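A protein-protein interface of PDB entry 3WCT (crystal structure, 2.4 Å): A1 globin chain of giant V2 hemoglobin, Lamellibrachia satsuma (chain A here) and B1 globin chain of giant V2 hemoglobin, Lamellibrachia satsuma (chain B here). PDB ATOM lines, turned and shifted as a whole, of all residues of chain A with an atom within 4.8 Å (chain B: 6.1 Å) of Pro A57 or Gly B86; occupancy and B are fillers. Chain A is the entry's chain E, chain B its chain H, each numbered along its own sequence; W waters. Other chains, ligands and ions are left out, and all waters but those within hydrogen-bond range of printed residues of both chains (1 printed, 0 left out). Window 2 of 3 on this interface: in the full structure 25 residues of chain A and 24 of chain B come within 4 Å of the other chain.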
ATOM      1  N   ARG A  55      -3.093   4.377 -29.418  1.00  0.00           N
ATOM      2  CA  ARG A  55      -1.984   3.967 -28.563  1.00  0.00           C
ATOM      3  C   ARG A  55      -2.426   3.045 -27.428  1.00  0.00           C
ATOM      4  O   ARG A  55      -1.730   2.895 -26.416  1.00  0.00           O
ATOM      5  CB  ARG A  55      -1.252   5.199 -28.004  1.00  0.00           C
ATOM      6  CG  ARG A  55      -0.993   6.308 -29.033  1.00  0.00           C
ATOM      7  CD  ARG A  55      -0.467   5.764 -30.363  1.00  0.00           C
ATOM      8  NE  ARG A  55       0.990   5.649 -30.423  1.00  0.00           N
ATOM      9  CZ  ARG A  55       1.817   6.670 -30.642  1.00  0.00           C
ATOM     10  NH1 ARG A  55       3.126   6.468 -30.680  1.00  0.00           N
ATOM     11  NH2 ARG A  55       1.335   7.895 -30.829  1.00  0.00           N
ATOM     12  N   SER A  56      -3.588   2.427 -27.610  1.00  0.00           N
ATOM     13  CA  SER A  56      -4.128   1.490 -26.630  1.00  0.00           C
ATOM     14  C   SER A  56      -3.526   0.119 -26.925  1.00  0.00           C
ATOM     15  O   SER A  56      -3.165  -0.171 -28.067  1.00  0.00           O
ATOM     16  CB  SER A  56      -5.645   1.399 -26.763  1.00  0.00           C
ATOM     17  OG  SER A  56      -6.000   0.840 -28.018  1.00  0.00           O
ATOM     18  N   PRO A  57      -3.419  -0.750 -25.906  1.00  0.00           N
ATOM     19  CA  PRO A  57      -2.847  -2.079 -26.147  1.00  0.00           C
ATOM     20  C   PRO A  57      -3.590  -2.865 -27.217  1.00  0.00           C
ATOM     21  O   PRO A  57      -2.980  -3.590 -27.998  1.00  0.00           O
ATOM     22  CB  PRO A  57      -2.930  -2.743 -24.773  1.00  0.00           C
ATOM     23  CG  PRO A  57      -4.127  -2.092 -24.155  1.00  0.00           C
ATOM     24  CD  PRO A  57      -3.912  -0.639 -24.521  1.00  0.00           C
ATOM     25  N   GLN A  58      -4.909  -2.712 -27.254  1.00  0.00           N
ATOM     26  CA  GLN A  58      -5.739  -3.421 -28.219  1.00  0.00           C
ATOM     27  C   GLN A  58      -5.420  -3.068 -29.667  1.00  0.00           C
ATOM     28  O   GLN A  58      -5.386  -3.948 -30.528  1.00  0.00           O
ATOM     29  CB  GLN A  58      -7.225  -3.146 -27.962  1.00  0.00           C
ATOM     30  CG  GLN A  58      -7.793  -3.687 -26.648  1.00  0.00           C
ATOM     31  CD  GLN A  58      -7.361  -2.876 -25.437  1.00  0.00           C
ATOM     32  OE1 GLN A  58      -7.281  -1.645 -25.491  1.00  0.00           O
ATOM     33  NE2 GLN A  58      -7.095  -3.563 -24.331  1.00  0.00           N
ATOM     34  N   PHE A  59      -5.201  -1.786 -29.946  1.00  0.00           N
ATOM     35  CA  PHE A  59      -4.903  -1.390 -31.311  1.00  0.00           C
ATOM     36  C   PHE A  59      -3.447  -1.674 -31.636  1.00  0.00           C
ATOM     37  O   PHE A  59      -3.129  -2.093 -32.746  1.00  0.00           O
ATOM     38  CB  PHE A  59      -5.222   0.094 -31.543  1.00  0.00           C
ATOM     39  CG  PHE A  59      -5.252   0.483 -33.005  1.00  0.00           C
ATOM     40  CD1 PHE A  59      -4.207   1.208 -33.575  1.00  0.00           C
ATOM     41  CD2 PHE A  59      -6.313   0.092 -33.821  1.00  0.00           C
ATOM     42  CE1 PHE A  59      -4.219   1.534 -34.931  1.00  0.00           C
ATOM     43  CE2 PHE A  59      -6.331   0.417 -35.179  1.00  0.00           C
ATOM     44  CZ  PHE A  59      -5.281   1.138 -35.732  1.00  0.00           C
ATOM     45  N   LYS A  60      -2.563  -1.451 -30.668  1.00  0.00           N
ATOM     46  CA  LYS A  60      -1.141  -1.711 -30.879  1.00  0.00           C
ATOM     47  C   LYS A  60      -0.932  -3.195 -31.168  1.00  0.00           C
ATOM     48  O   LYS A  60      -0.053  -3.567 -31.935  1.00  0.00           O
ATOM     49  CB  LYS A  60      -0.322  -1.277 -29.663  1.00  0.00           C
ATOM     50  CG  LYS A  60      -0.205   0.242 -29.524  1.00  0.00           C
ATOM     51  CD  LYS A  60       0.900   0.658 -28.553  1.00  0.00           C
ATOM     52  CE  LYS A  60       0.590   0.239 -27.125  1.00  0.00           C
ATOM     53  NZ  LYS A  60       1.694   0.583 -26.174  1.00  0.00           N
ATOM     54  N   ALA A  61      -1.751  -4.037 -30.551  1.00  0.00           N
ATOM     55  CA  ALA A  61      -1.672  -5.472 -30.770  1.00  0.00           C
ATOM     56  C   ALA A  61      -2.109  -5.700 -32.208  1.00  0.00           C
ATOM     57  O   ALA A  61      -1.576  -6.569 -32.907  1.00  0.00           O
ATOM     58  CB  ALA A  61      -2.608  -6.210 -29.816  1.00  0.00           C
ATOM     59  N   PHE B   3       5.520 -10.641 -17.301  1.00  0.00           N
ATOM     60  CA  PHE B   3       6.199 -11.673 -18.080  1.00  0.00           C
ATOM     61  C   PHE B   3       7.597 -11.942 -17.532  1.00  0.00           C
ATOM     62  O   PHE B   3       7.759 -12.756 -16.616  1.00  0.00           O
ATOM     63  CB  PHE B   3       6.271 -11.242 -19.546  1.00  0.00           C
ATOM     64  CG  PHE B   3       4.928 -11.157 -20.209  1.00  0.00           C
ATOM     65  CD1 PHE B   3       4.327 -12.294 -20.731  1.00  0.00           C
ATOM     66  CD2 PHE B   3       4.230  -9.956 -20.246  1.00  0.00           C
ATOM     67  CE1 PHE B   3       3.046 -12.238 -21.278  1.00  0.00           C
ATOM     68  CE2 PHE B   3       2.952  -9.890 -20.789  1.00  0.00           C
ATOM     69  CZ  PHE B   3       2.357 -11.035 -21.306  1.00  0.00           C
ATOM     70  N   ASP B  84       6.861  -4.680 -23.372  1.00  0.00           N
ATOM     71  CA  ASP B  84       5.662  -3.849 -23.473  1.00  0.00           C
ATOM     72  C   ASP B  84       4.506  -4.721 -22.987  1.00  0.00           C
ATOM     73  O   ASP B  84       3.603  -5.054 -23.763  1.00  0.00           O
ATOM     74  CB  ASP B  84       5.403  -3.421 -24.916  1.00  0.00           C
ATOM     75  CG  ASP B  84       4.244  -2.440 -25.033  1.00  0.00           C
ATOM     76  OD1 ASP B  84       3.223  -2.617 -24.327  1.00  0.00           O
ATOM     77  OD2 ASP B  84       4.348  -1.493 -25.842  1.00  0.00           O
ATOM     78  N   ALA B  85       4.556  -5.088 -21.706  1.00  0.00           N
ATOM     79  CA  ALA B  85       3.558  -5.955 -21.072  1.00  0.00           C
ATOM     80  C   ALA B  85       2.115  -5.622 -21.403  1.00  0.00           C
ATOM     81  O   ALA B  85       1.275  -6.508 -21.453  1.00  0.00           O
ATOM     82  CB  ALA B  85       3.750  -5.953 -19.548  1.00  0.00           C
ATOM     83  N   GLY B  86       1.830  -4.345 -21.626  1.00  0.00           N
ATOM     84  CA  GLY B  86       0.473  -3.944 -21.949  1.00  0.00           C
ATOM     85  C   GLY B  86      -0.005  -4.521 -23.272  1.00  0.00           C
ATOM     86  O   GLY B  86      -1.062  -5.144 -23.340  1.00  0.00           O
ATOM     87  N   THR B  87       0.780  -4.314 -24.323  1.00  0.00           N
ATOM     88  CA  THR B  87       0.434  -4.809 -25.646  1.00  0.00           C
ATOM     89  C   THR B  87       0.586  -6.322 -25.741  1.00  0.00           C
ATOM     90  O   THR B  87      -0.238  -6.999 -26.366  1.00  0.00           O
ATOM     91  CB  THR B  87       1.322  -4.161 -26.714  1.00  0.00           C
ATOM     92  OG1 THR B  87       1.135  -2.742 -26.685  1.00  0.00           O
ATOM     93  CG2 THR B  87       0.971  -4.689 -28.094  1.00  0.00           C
ATOM     94  N   LEU B  88       1.640  -6.848 -25.123  1.00  0.00           N
ATOM     95  CA  LEU B  88       1.898  -8.283 -25.145  1.00  0.00           C
ATOM     96  C   LEU B  88       0.750  -9.019 -24.472  1.00  0.00           C
ATOM     97  O   LEU B  88       0.395 -10.130 -24.872  1.00  0.00           O
ATOM     98  CB  LEU B  88       3.225  -8.616 -24.442  1.00  0.00           C
ATOM     99  CG  LEU B  88       3.634 -10.097 -24.365  1.00  0.00           C
ATOM    100  CD1 LEU B  88       3.668 -10.705 -25.752  1.00  0.00           C
ATOM    101  CD2 LEU B  88       4.997 -10.225 -23.712  1.00  0.00           C
ATOM    102  N   THR B  89       0.168  -8.401 -23.448  1.00  0.00           N
ATOM    103  CA  THR B  89      -0.956  -9.019 -22.745  1.00  0.00           C
ATOM    104  C   THR B  89      -2.111  -9.158 -23.730  1.00  0.00           C
ATOM    105  O   THR B  89      -2.748 -10.204 -23.823  1.00  0.00           O
ATOM    106  CB  THR B  89      -1.426  -8.155 -21.564  1.00  0.00           C
ATOM    107  OG1 THR B  89      -0.354  -8.021 -20.622  1.00  0.00           O
ATOM    108  CG2 THR B  89      -2.635  -8.807 -20.867  1.00  0.00           C
ATOM    109  N   SER B  90      -2.371  -8.088 -24.469  1.00  0.00           N
ATOM    110  CA  SER B  90      -3.441  -8.097 -25.445  1.00  0.00           C
ATOM    111  C   SER B  90      -3.087  -9.063 -26.580  1.00  0.00           C
ATOM    112  O   SER B  90      -3.945  -9.793 -27.071  1.00  0.00           O
ATOM    113  CB  SER B  90      -3.669  -6.685 -25.982  1.00  0.00           C
ATOM    114  OG  SER B  90      -4.753  -6.662 -26.897  1.00  0.00           O
ATOM    115  N   LEU B  91      -1.820  -9.079 -26.988  1.00  0.00           N
ATOM    116  CA  LEU B  91      -1.392  -9.981 -28.052  1.00  0.00           C
ATOM    117  C   LEU B  91      -1.559 -11.451 -27.656  1.00  0.00           C
ATOM    118  O   LEU B  91      -2.053 -12.257 -28.451  1.00  0.00           O
ATOM    119  CB  LEU B  91       0.060  -9.701 -28.430  1.00  0.00           C
ATOM    120  CG  LEU B  91       0.283  -8.523 -29.382  1.00  0.00           C
ATOM    121  CD1 LEU B  91       1.770  -8.230 -29.512  1.00  0.00           C
ATOM    122  CD2 LEU B  91      -0.312  -8.867 -30.742  1.00  0.00           C
HETATM  123  O   HOH W   1      -7.285  -6.564 -25.456  1.00  0.00           O
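OD2 of Asp B84 is in salt-bridge range of NZ of Lys A60 (3.4 Å). The side-chain hydroxyl (OG1) of Thr B87 lies close to the side-chain amino group (NZ) of Lys A60 (3.4 Å).
OD1 of Asp B84 lies close to N of Gly B86, at 3.5 Å. OD1 of Asp B84 is in hydrogen-bond range of N of Thr B87 (3.0 Å).
CB of Pro A57 touches O of Gly B86 (3.4 Å). O of Pro A57 touches OG of Ser B90, at 3.7 Å. Gln A58 touches Ser B90. Ala A61 touches Thr B87 (N to CG2, 3.7 Å). Ser B90 touches Ala A61. O of Ala A61 touches CD2 of Leu B91 (3.4 Å).
Pro A57 touches two residues of chain B. Gly B86 touches just one residue of chain A: Pro A57. Of the printed residues of chain A, Thr B87 touches Lys A60 (3.1 Å) and Ala A61 (3.7 Å). Of the printed residues of chain B, Lys A60 touches Asp B84 (3.4 Å) and Thr B87 (3.1 Å). Of the printed residues of chain B, Gln A58 touches Ser B90. Printed residues of chain A within 4 Å of Leu B91: Ala A61 (3.4 Å). Of the printed residues of chain A, Asp B84 touches Lys A60 (3.4 Å). Ser A56 touches none of the printed residues of chain B. Phe A59 touches none of the printed residues of chain B. The nearest printed residue of chain A that does not touch Gly B86 is Gln A58 (6.0 Å). The nearest printed residue of chain A that does not touch Ser B90 is Phe A59 (5.8 Å).
Hydrophobic or aromatic side chains of chain B within 4 Å of the printed part of chain A: Leu B91.
Water W1 lies within hydrogen-bond range of the side-chain hydroxyl (OG) of Ser B90 and the side-chain amide nitrogen (NE2) of Gln A58.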
